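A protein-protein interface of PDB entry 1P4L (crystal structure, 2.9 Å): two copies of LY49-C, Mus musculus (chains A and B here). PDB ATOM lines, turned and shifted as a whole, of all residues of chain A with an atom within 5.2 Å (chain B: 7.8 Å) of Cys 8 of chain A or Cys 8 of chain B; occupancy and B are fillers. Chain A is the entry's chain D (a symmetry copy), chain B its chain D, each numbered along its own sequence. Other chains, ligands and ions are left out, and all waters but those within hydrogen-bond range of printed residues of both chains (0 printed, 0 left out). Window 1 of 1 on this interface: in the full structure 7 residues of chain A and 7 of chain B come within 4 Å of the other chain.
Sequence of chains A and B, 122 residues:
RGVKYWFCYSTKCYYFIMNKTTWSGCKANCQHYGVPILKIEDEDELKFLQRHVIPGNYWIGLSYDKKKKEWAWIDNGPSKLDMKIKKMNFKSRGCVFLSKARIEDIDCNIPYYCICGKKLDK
The backbone NH of Cys 8 of chain A is in hydrogen-bond range of the backbone carbonyl oxygen of Ser 10 of chain B, at 2.4 Å. N of Cys 8 of chain B sits at hydrogen-bond distance from O of Ser 10 of chain A (2.4 Å).
The backbone carbonyl oxygen (O) of Phe 7 of chain B is in hydrogen-bond range of the backbone NH (N) of Tyr 14 of chain B. The backbone carbonyl oxygen (O) of Phe 7 of chain A sits at hydrogen-bond distance from the backbone NH (N) of Tyr 14 of chain A (2.9 Å). The side-chain sulfur (SG) of Cys 8 of chain B is disulfide-bonded to the side-chain sulfur (SG) of Cys 13 of chain B, at 2.0 Å. The backbone carbonyl oxygen (O) of Thr 11 of chain A lies within hydrogen-bond range of the backbone NH (N) of Leu 120 of chain A, at 3.4 Å. O of Thr 11 of chain B sits at hydrogen-bond distance from N of Leu 120 of chain B, at 3.4 Å. The side-chain sulfur (SG) of Cys 8 of chain A is disulfide-bonded to the side-chain sulfur (SG) of Cys 13 of chain A, at 2.0 Å.
CH2 of Trp 6 of chain A touches OG1 of Thr 11 of chain B, 3.3 Å away. CE1 of Tyr 9 of chain B touches CZ of Phe 7 of chain A (3.5 Å). Phe 7 of chain A touches Ser 10 of chain B (C to O, 3.4 Å). Cys 8 of chain B touches Cys 8 of chain A. Tyr 9 of chain B touches Cys 8 of chain A. Tyr 9 of chain A touches Phe 7 of chain B (CE1 to CZ, 3.5 Å). Tyr 9 of chain A touches Cys 8 of chain B (CA to O, 3.2 Å). Phe 7 of chain B touches Ser 10 of chain A (C to O, 3.4 Å). Trp 6 of chain B touches Thr 11 of chain A. Cys 8 of chain B touches Leu 120 of chain A.
Cys 8 of chain A touches four residues of chain B. Of the printed residues of chain B, Leu 120 of chain A touches Cys 8. Printed residues of chain A within 4 Å of Trp 6 of chain B: Thr 11. Of the printed residues of chain A, Tyr 9 of chain B touches Phe 7 (3.5 Å) and Cys 8 (3.2 Å). Printed residues of chain A within 4 Å of Thr 11 of chain B: Trp 6. The nearest residue of chain B that does not touch Cys 8 of chain A is Thr 11 of chain B (4.6 Å).
Of the 16 printed residues of chain B, 7 touch a printed residue of chain A. Among the printed residues, no Asp or Glu carboxylate lies within 4 Å of a Lys or Arg side-chain nitrogen of the other chain.
Trp 6 of chain A touches Thr 11 of chain B, and with the chains exchanged Thr 11 of chain A touches Trp 6 of chain B. Phe 7 of chain A touches Tyr 9 of chain B, and with the chains exchanged Tyr 9 of chain A touches Phe 7 of chain B. Cys 8 of chain A touches Tyr 9 of chain B, and with the chains exchanged Tyr 9 of chain A touches Cys 8 of chain B. Cys 8 of chain A touches Leu 120 of chain B, and with the chains exchanged Leu 120 of chain A touches Cys 8 of chain B. Positions printed for both chains: 6, 7, 8, 9, 10, 11, 12, 13, 14 and 120.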
ATOM      1  N   TRP A   6     -18.065  37.047  -4.031  1.00  0.00           N
ATOM      2  CA  TRP A   6     -17.225  35.959  -4.570  1.00  0.00           C
ATOM      3  C   TRP A   6     -17.868  34.587  -4.244  1.00  0.00           C
ATOM      4  O   TRP A   6     -18.440  34.370  -3.170  1.00  0.00           O
ATOM      5  CB  TRP A   6     -15.767  36.034  -4.089  1.00  0.00           C
ATOM      6  CG  TRP A   6     -15.695  35.941  -2.655  1.00  0.00           C
ATOM      7  CD1 TRP A   6     -15.932  36.959  -1.754  1.00  0.00           C
ATOM      8  CD2 TRP A   6     -15.541  34.740  -1.891  1.00  0.00           C
ATOM      9  NE1 TRP A   6     -15.945  36.453  -0.466  1.00  0.00           N
ATOM     10  CE2 TRP A   6     -15.710  35.097  -0.516  1.00  0.00           C
ATOM     11  CE3 TRP A   6     -15.290  33.396  -2.228  1.00  0.00           C
ATOM     12  CZ2 TRP A   6     -15.634  34.151   0.529  1.00  0.00           C
ATOM     13  CZ3 TRP A   6     -15.213  32.441  -1.185  1.00  0.00           C
ATOM     14  CH2 TRP A   6     -15.387  32.833   0.180  1.00  0.00           C
ATOM     15  N   PHE A   7     -17.758  33.687  -5.216  1.00  0.00           N
ATOM     16  CA  PHE A   7     -18.363  32.371  -5.160  1.00  0.00           C
ATOM     17  C   PHE A   7     -17.469  31.356  -5.907  1.00  0.00           C
ATOM     18  O   PHE A   7     -16.972  31.623  -7.002  1.00  0.00           O
ATOM     19  CB  PHE A   7     -19.771  32.533  -5.773  1.00  0.00           C
ATOM     20  CG  PHE A   7     -20.466  31.261  -6.139  1.00  0.00           C
ATOM     21  CD1 PHE A   7     -21.747  31.013  -5.672  1.00  0.00           C
ATOM     22  CD2 PHE A   7     -19.888  30.356  -7.017  1.00  0.00           C
ATOM     23  CE1 PHE A   7     -22.443  29.887  -6.075  1.00  0.00           C
ATOM     24  CE2 PHE A   7     -20.575  29.229  -7.425  1.00  0.00           C
ATOM     25  CZ  PHE A   7     -21.859  28.994  -6.952  1.00  0.00           C
ATOM     26  N   CYS A   8     -17.270  30.195  -5.292  1.00  0.00           N
ATOM     27  CA  CYS A   8     -16.431  29.140  -5.848  1.00  0.00           C
ATOM     28  C   CYS A   8     -17.224  28.060  -6.541  1.00  0.00           C
ATOM     29  O   CYS A   8     -18.324  27.717  -6.123  1.00  0.00           O
ATOM     30  CB  CYS A   8     -15.628  28.473  -4.741  1.00  0.00           C
ATOM     31  SG  CYS A   8     -14.539  29.593  -3.826  1.00  0.00           S
ATOM     32  N   TYR A   9     -16.644  27.513  -7.599  1.00  0.00           N
ATOM     33  CA  TYR A   9     -17.273  26.425  -8.340  1.00  0.00           C
ATOM     34  C   TYR A   9     -16.213  25.438  -8.821  1.00  0.00           C
ATOM     35  O   TYR A   9     -15.223  25.809  -9.452  1.00  0.00           O
ATOM     36  CB  TYR A   9     -18.065  26.935  -9.540  1.00  0.00           C
ATOM     37  CG  TYR A   9     -18.718  25.815 -10.311  1.00  0.00           C
ATOM     38  CD1 TYR A   9     -19.795  25.107  -9.774  1.00  0.00           C
ATOM     39  CD2 TYR A   9     -18.253  25.451 -11.576  1.00  0.00           C
ATOM     40  CE1 TYR A   9     -20.402  24.063 -10.482  1.00  0.00           C
ATOM     41  CE2 TYR A   9     -18.845  24.409 -12.294  1.00  0.00           C
ATOM     42  CZ  TYR A   9     -19.920  23.720 -11.743  1.00  0.00           C
ATOM     43  OH  TYR A   9     -20.505  22.694 -12.450  1.00  0.00           O
ATOM     44  N   SER A  10     -16.451  24.169  -8.520  1.00  0.00           N
ATOM     45  CA  SER A  10     -15.535  23.105  -8.880  1.00  0.00           C
ATOM     46  C   SER A  10     -14.188  23.295  -8.185  1.00  0.00           C
ATOM     47  O   SER A  10     -14.085  23.216  -6.960  1.00  0.00           O
ATOM     48  CB  SER A  10     -15.336  23.066 -10.387  1.00  0.00           C
ATOM     49  OG  SER A  10     -14.407  22.057 -10.729  1.00  0.00           O
ATOM     50  N   THR A  11     -13.156  23.555  -8.976  1.00  0.00           N
ATOM     51  CA  THR A  11     -11.806  23.759  -8.453  1.00  0.00           C
ATOM     52  C   THR A  11     -11.277  25.144  -8.889  1.00  0.00           C
ATOM     53  O   THR A  11     -10.136  25.297  -9.330  1.00  0.00           O
ATOM     54  CB  THR A  11     -10.901  22.571  -8.919  1.00  0.00           C
ATOM     55  OG1 THR A  11     -11.090  21.468  -8.022  1.00  0.00           O
ATOM     56  CG2 THR A  11      -9.442  22.936  -8.939  1.00  0.00           C
ATOM     57  N   LYS A  12     -12.146  26.145  -8.750  1.00  0.00           N
ATOM     58  CA  LYS A  12     -11.853  27.537  -9.101  1.00  0.00           C
ATOM     59  C   LYS A  12     -12.850  28.428  -8.379  1.00  0.00           C
ATOM     60  O   LYS A  12     -13.957  28.006  -8.067  1.00  0.00           O
ATOM     61  CB  LYS A  12     -12.030  27.792 -10.606  1.00  0.00           C
ATOM     62  CG  LYS A  12     -11.101  27.021 -11.538  1.00  0.00           C
ATOM     63  CD  LYS A  12     -11.318  27.386 -13.017  1.00  0.00           C
ATOM     64  CE  LYS A  12     -11.058  28.864 -13.285  1.00  0.00           C
ATOM     65  NZ  LYS A  12     -10.913  29.158 -14.745  1.00  0.00           N
ATOM     66  N   CYS A  13     -12.465  29.662  -8.102  1.00  0.00           N
ATOM     67  CA  CYS A  13     -13.400  30.576  -7.470  1.00  0.00           C
ATOM     68  C   CYS A  13     -13.446  31.801  -8.334  1.00  0.00           C
ATOM     69  O   CYS A  13     -12.490  32.107  -9.052  1.00  0.00           O
ATOM     70  CB  CYS A  13     -12.964  30.967  -6.073  1.00  0.00           C
ATOM     71  SG  CYS A  13     -12.840  29.558  -4.941  1.00  0.00           S
ATOM     72  N   TYR A  14     -14.556  32.512  -8.264  1.00  0.00           N
ATOM     73  CA  TYR A  14     -14.705  33.685  -9.082  1.00  0.00           C
ATOM     74  C   TYR A  14     -15.031  34.908  -8.266  1.00  0.00           C
ATOM     75  O   TYR A  14     -15.424  34.826  -7.102  1.00  0.00           O
ATOM     76  CB  TYR A  14     -15.814  33.462 -10.112  1.00  0.00           C
ATOM     77  CG  TYR A  14     -15.598  32.260 -10.990  1.00  0.00           C
ATOM     78  CD1 TYR A  14     -15.900  30.979 -10.546  1.00  0.00           C
ATOM     79  CD2 TYR A  14     -15.053  32.401 -12.257  1.00  0.00           C
ATOM     80  CE1 TYR A  14     -15.660  29.872 -11.346  1.00  0.00           C
ATOM     81  CE2 TYR A  14     -14.807  31.305 -13.061  1.00  0.00           C
ATOM     82  CZ  TYR A  14     -15.108  30.045 -12.600  1.00  0.00           C
ATOM     83  OH  TYR A  14     -14.824  28.955 -13.385  1.00  0.00           O
ATOM     84  N   LEU A 120      -8.084  27.652  -8.052  1.00  0.00           N
ATOM     85  CA  LEU A 120      -7.605  27.222  -6.737  1.00  0.00           C
ATOM     86  C   LEU A 120      -6.476  26.200  -6.766  1.00  0.00           C
ATOM     87  O   LEU A 120      -5.499  26.313  -6.022  1.00  0.00           O
ATOM     88  CB  LEU A 120      -8.761  26.625  -5.937  1.00  0.00           C
ATOM     89  CG  LEU A 120      -9.966  27.505  -5.622  1.00  0.00           C
ATOM     90  CD1 LEU A 120     -10.997  26.678  -4.872  1.00  0.00           C
ATOM     91  CD2 LEU A 120      -9.533  28.700  -4.793  1.00  0.00           C
ATOM     92  N   TYR B   5     -12.158  12.640  -4.577  1.00  0.00           N
ATOM     93  CA  TYR B   5     -12.418  13.721  -5.528  1.00  0.00           C
ATOM     94  C   TYR B   5     -12.849  14.925  -4.669  1.00  0.00           C
ATOM     95  O   TYR B   5     -13.656  14.760  -3.733  1.00  0.00           O
ATOM     96  CB  TYR B   5     -13.601  13.312  -6.442  1.00  0.00           C
ATOM     97  CG  TYR B   5     -13.968  14.277  -7.562  1.00  0.00           C
ATOM     98  CD1 TYR B   5     -14.220  15.643  -7.306  1.00  0.00           C
ATOM     99  CD2 TYR B   5     -14.030  13.820  -8.917  1.00  0.00           C
ATOM    100  CE1 TYR B   5     -14.514  16.558  -8.377  1.00  0.00           C
ATOM    101  CE2 TYR B   5     -14.329  14.720 -10.027  1.00  0.00           C
ATOM    102  CZ  TYR B   5     -14.562  16.094  -9.749  1.00  0.00           C
ATOM    103  OH  TYR B   5     -14.777  16.983 -10.835  1.00  0.00           O
ATOM    104  N   TRP B   6     -12.292  16.111  -4.922  1.00  0.00           N
ATOM    105  CA  TRP B   6     -12.813  17.278  -4.184  1.00  0.00           C
ATOM    106  C   TRP B   6     -13.244  18.383  -5.182  1.00  0.00           C
ATOM    107  O   TRP B   6     -12.608  18.616  -6.216  1.00  0.00           O
ATOM    108  CB  TRP B   6     -11.826  17.812  -3.133  1.00  0.00           C
ATOM    109  CG  TRP B   6     -10.596  18.229  -3.751  1.00  0.00           C
ATOM    110  CD1 TRP B   6      -9.560  17.410  -4.152  1.00  0.00           C
ATOM    111  CD2 TRP B   6     -10.292  19.545  -4.229  1.00  0.00           C
ATOM    112  NE1 TRP B   6      -8.630  18.146  -4.865  1.00  0.00           N
ATOM    113  CE2 TRP B   6      -9.049  19.456  -4.930  1.00  0.00           C
ATOM    114  CE3 TRP B   6     -10.949  20.788  -4.145  1.00  0.00           C
ATOM    115  CZ2 TRP B   6      -8.444  20.571  -5.549  1.00  0.00           C
ATOM    116  CZ3 TRP B   6     -10.348  21.911  -4.764  1.00  0.00           C
ATOM    117  CH2 TRP B   6      -9.103  21.787  -5.459  1.00  0.00           C
ATOM    118  N   PHE B   7     -14.348  19.035  -4.832  1.00  0.00           N
ATOM    119  CA  PHE B   7     -14.978  20.044  -5.662  1.00  0.00           C
ATOM    120  C   PHE B   7     -15.634  21.118  -4.765  1.00  0.00           C
ATOM    121  O   PHE B   7     -16.298  20.809  -3.776  1.00  0.00           O
ATOM    122  CB  PHE B   7     -15.979  19.281  -6.558  1.00  0.00           C
ATOM    123  CG  PHE B   7     -16.990  20.128  -7.260  1.00  0.00           C
ATOM    124  CD1 PHE B   7     -17.153  20.017  -8.632  1.00  0.00           C
ATOM    125  CD2 PHE B   7     -17.840  20.966  -6.552  1.00  0.00           C
ATOM    126  CE1 PHE B   7     -18.147  20.721  -9.287  1.00  0.00           C
ATOM    127  CE2 PHE B   7     -18.835  21.674  -7.199  1.00  0.00           C
ATOM    128  CZ  PHE B   7     -18.990  21.550  -8.573  1.00  0.00           C
ATOM    129  N   CYS B   8     -15.427  22.380  -5.126  1.00  0.00           N
ATOM    130  CA  CYS B   8     -15.952  23.513  -4.375  1.00  0.00           C
ATOM    131  C   CYS B   8     -17.217  24.081  -4.970  1.00  0.00           C
ATOM    132  O   CYS B   8     -17.387  24.107  -6.184  1.00  0.00           O
ATOM    133  CB  CYS B   8     -14.926  24.636  -4.336  1.00  0.00           C
ATOM    134  SG  CYS B   8     -13.345  24.181  -3.578  1.00  0.00           S
ATOM    135  N   TYR B   9     -18.098  24.553  -4.101  1.00  0.00           N
ATOM    136  CA  TYR B   9     -19.344  25.173  -4.534  1.00  0.00           C
ATOM    137  C   TYR B   9     -19.700  26.336  -3.612  1.00  0.00           C
ATOM    138  O   TYR B   9     -19.744  26.200  -2.389  1.00  0.00           O
ATOM    139  CB  TYR B   9     -20.501  24.178  -4.555  1.00  0.00           C
ATOM    140  CG  TYR B   9     -21.794  24.814  -5.002  1.00  0.00           C
ATOM    141  CD1 TYR B   9     -21.978  25.207  -6.330  1.00  0.00           C
ATOM    142  CD2 TYR B   9     -22.833  25.035  -4.097  1.00  0.00           C
ATOM    143  CE1 TYR B   9     -23.173  25.802  -6.750  1.00  0.00           C
ATOM    144  CE2 TYR B   9     -24.031  25.630  -4.501  1.00  0.00           C
ATOM    145  CZ  TYR B   9     -24.196  26.010  -5.828  1.00  0.00           C
ATOM    146  OH  TYR B   9     -25.376  26.597  -6.227  1.00  0.00           O
ATOM    147  N   SER B  10     -19.964  27.480  -4.227  1.00  0.00           N
ATOM    148  CA  SER B  10     -20.295  28.689  -3.501  1.00  0.00           C
ATOM    149  C   SER B  10     -19.126  29.126  -2.620  1.00  0.00           C
ATOM    150  O   SER B  10     -18.059  29.496  -3.112  1.00  0.00           O
ATOM    151  CB  SER B  10     -21.532  28.470  -2.644  1.00  0.00           C
ATOM    152  OG  SER B  10     -21.824  29.638  -1.903  1.00  0.00           O
ATOM    153  N   THR B  11     -19.331  29.072  -1.311  1.00  0.00           N
ATOM    154  CA  THR B  11     -18.305  29.460  -0.345  1.00  0.00           C
ATOM    155  C   THR B  11     -18.007  28.282   0.608  1.00  0.00           C
ATOM    156  O   THR B  11     -17.906  28.437   1.826  1.00  0.00           O
ATOM    157  CB  THR B  11     -18.773  30.757   0.394  1.00  0.00           C
ATOM    158  OG1 THR B  11     -18.450  31.894  -0.419  1.00  0.00           O
ATOM    159  CG2 THR B  11     -18.118  30.918   1.738  1.00  0.00           C
ATOM    160  N   LYS B  12     -17.870  27.098   0.010  1.00  0.00           N
ATOM    161  CA  LYS B  12     -17.586  25.850   0.723  1.00  0.00           C
ATOM    162  C   LYS B  12     -17.033  24.848  -0.277  1.00  0.00           C
ATOM    163  O   LYS B  12     -17.324  24.922  -1.465  1.00  0.00           O
ATOM    164  CB  LYS B  12     -18.862  25.232   1.318  1.00  0.00           C
ATOM    165  CG  LYS B  12     -19.579  26.056   2.382  1.00  0.00           C
ATOM    166  CD  LYS B  12     -20.810  25.331   2.955  1.00  0.00           C
ATOM    167  CE  LYS B  12     -20.437  24.010   3.620  1.00  0.00           C
ATOM    168  NZ  LYS B  12     -21.539  23.478   4.479  1.00  0.00           N
ATOM    169  N   CYS B  13     -16.228  23.911   0.192  1.00  0.00           N
ATOM    170  CA  CYS B  13     -15.720  22.890  -0.708  1.00  0.00           C
ATOM    171  C   CYS B  13     -16.062  21.568  -0.087  1.00  0.00           C
ATOM    172  O   CYS B  13     -16.217  21.462   1.133  1.00  0.00           O
ATOM    173  CB  CYS B  13     -14.220  22.982  -0.892  1.00  0.00           C
ATOM    174  SG  CYS B  13     -13.680  24.556  -1.609  1.00  0.00           S
ATOM    175  N   TYR B  14     -16.175  20.553  -0.924  1.00  0.00           N
ATOM    176  CA  TYR B  14     -16.533  19.253  -0.423  1.00  0.00           C
ATOM    177  C   TYR B  14     -15.534  18.198  -0.817  1.00  0.00           C
ATOM    178  O   TYR B  14     -14.707  18.388  -1.709  1.00  0.00           O
ATOM    179  CB  TYR B  14     -17.913  18.856  -0.952  1.00  0.00           C
ATOM    180  CG  TYR B  14     -19.001  19.842  -0.619  1.00  0.00           C
ATOM    181  CD1 TYR B  14     -19.170  21.005  -1.359  1.00  0.00           C
ATOM    182  CD2 TYR B  14     -19.839  19.627   0.464  1.00  0.00           C
ATOM    183  CE1 TYR B  14     -20.148  21.927  -1.021  1.00  0.00           C
ATOM    184  CE2 TYR B  14     -20.814  20.542   0.810  1.00  0.00           C
ATOM    185  CZ  TYR B  14     -20.962  21.690   0.069  1.00  0.00           C
ATOM    186  OH  TYR B  14     -21.905  22.616   0.441  1.00  0.00           O
ATOM    187  N   TYR B  15     -15.612  17.080  -0.115  1.00  0.00           N
ATOM    188  CA  TYR B  15     -14.775  15.942  -0.415  1.00  0.00           C
ATOM    189  C   TYR B  15     -15.756  14.826  -0.689  1.00  0.00           C
ATOM    190  O   TYR B  15     -16.705  14.620   0.076  1.00  0.00           O
ATOM    191  CB  TYR B  15     -13.871  15.593   0.760  1.00  0.00           C
ATOM    192  CG  TYR B  15     -12.396  15.844   0.474  1.00  0.00           C
ATOM    193  CD1 TYR B  15     -11.731  16.966   1.000  1.00  0.00           C
ATOM    194  CD2 TYR B  15     -11.659  14.952  -0.317  1.00  0.00           C
ATOM    195  CE1 TYR B  15     -10.359  17.186   0.747  1.00  0.00           C
ATOM    196  CE2 TYR B  15     -10.294  15.160  -0.577  1.00  0.00           C
ATOM    197  CZ  TYR B  15      -9.647  16.274  -0.041  1.00  0.00           C
ATOM    198  OH  TYR B  15      -8.290  16.440  -0.265  1.00  0.00           O
ATOM    199  N   PHE B  16     -15.559  14.149  -1.811  1.00  0.00           N
ATOM    200  CA  PHE B  16     -16.436  13.060  -2.183  1.00  0.00           C
ATOM    201  C   PHE B  16     -15.609  11.799  -2.237  1.00  0.00           C
ATOM    202  O   PHE B  16     -14.870  11.573  -3.199  1.00  0.00           O
ATOM    203  CB  PHE B  16     -17.076  13.322  -3.544  1.00  0.00           C
ATOM    204  CG  PHE B  16     -18.079  14.430  -3.532  1.00  0.00           C
ATOM    205  CD1 PHE B  16     -17.677  15.751  -3.395  1.00  0.00           C
ATOM    206  CD2 PHE B  16     -19.431  14.154  -3.641  1.00  0.00           C
ATOM    207  CE1 PHE B  16     -18.620  16.783  -3.360  1.00  0.00           C
ATOM    208  CE2 PHE B  16     -20.375  15.178  -3.606  1.00  0.00           C
ATOM    209  CZ  PHE B  16     -19.970  16.492  -3.467  1.00  0.00           C
ATOM    210  N   PHE B  48     -28.096  21.425  -4.621  1.00  0.00           N
ATOM    211  CA  PHE B  48     -26.835  21.409  -5.338  1.00  0.00           C
ATOM    212  C   PHE B  48     -26.224  20.022  -5.189  1.00  0.00           C
ATOM    213  O   PHE B  48     -25.903  19.341  -6.168  1.00  0.00           O
ATOM    214  CB  PHE B  48     -25.876  22.440  -4.749  1.00  0.00           C
ATOM    215  CG  PHE B  48     -24.440  22.141  -5.043  1.00  0.00           C
ATOM    216  CD1 PHE B  48     -23.940  22.274  -6.335  1.00  0.00           C
ATOM    217  CD2 PHE B  48     -23.608  21.634  -4.052  1.00  0.00           C
ATOM    218  CE1 PHE B  48     -22.635  21.899  -6.641  1.00  0.00           C
ATOM    219  CE2 PHE B  48     -22.299  21.256  -4.348  1.00  0.00           C
ATOM    220  CZ  PHE B  48     -21.815  21.388  -5.649  1.00  0.00           C
ATOM    221  N   HIS B  52     -25.344  17.390  -8.075  1.00  0.00           N
ATOM    222  CA  HIS B  52     -23.941  17.156  -8.395  1.00  0.00           C
ATOM    223  C   HIS B  52     -23.523  15.696  -8.214  1.00  0.00           C
ATOM    224  O   HIS B  52     -22.903  15.093  -9.083  1.00  0.00           O
ATOM    225  CB  HIS B  52     -23.020  18.012  -7.532  1.00  0.00           C
ATOM    226  CG  HIS B  52     -21.591  17.586  -7.622  1.00  0.00           C
ATOM    227  ND1 HIS B  52     -20.897  17.071  -6.550  1.00  0.00           N
ATOM    228  CD2 HIS B  52     -20.769  17.475  -8.692  1.00  0.00           C
ATOM    229  CE1 HIS B  52     -19.711  16.652  -6.955  1.00  0.00           C
ATOM    230  NE2 HIS B  52     -19.611  16.885  -8.250  1.00  0.00           N
ATOM    231  N   LYS B 118     -16.301  21.509   3.851  1.00  0.00           N
ATOM    232  CA  LYS B 118     -15.368  22.474   4.424  1.00  0.00           C
ATOM    233  C   LYS B 118     -15.718  23.917   4.082  1.00  0.00           C
ATOM    234  O   LYS B 118     -15.339  24.430   3.026  1.00  0.00           O
ATOM    235  CB  LYS B 118     -13.939  22.183   3.961  1.00  0.00           C
ATOM    236  CG  LYS B 118     -12.896  23.064   4.625  1.00  0.00           C
ATOM    237  CD  LYS B 118     -11.841  23.561   3.636  1.00  0.00           C
ATOM    238  CE  LYS B 118     -11.005  22.430   3.039  1.00  0.00           C
ATOM    239  NZ  LYS B 118      -9.916  22.954   2.157  1.00  0.00           N
ATOM    240  N   LEU B 120     -15.229  27.261   3.511  1.00  0.00           N
ATOM    241  CA  LEU B 120     -14.064  28.101   3.226  1.00  0.00           C
ATOM    242  C   LEU B 120     -14.015  29.415   3.992  1.00  0.00           C
ATOM    243  O   LEU B 120     -12.969  29.807   4.515  1.00  0.00           O
ATOM    244  CB  LEU B 120     -14.013  28.422   1.734  1.00  0.00           C
ATOM    245  CG  LEU B 120     -13.893  27.271   0.739  1.00  0.00           C
ATOM    246  CD1 LEU B 120     -13.917  27.836  -0.671  1.00  0.00           C
ATOM    247  CD2 LEU B 120     -12.606  26.505   0.987  1.00  0.00           C
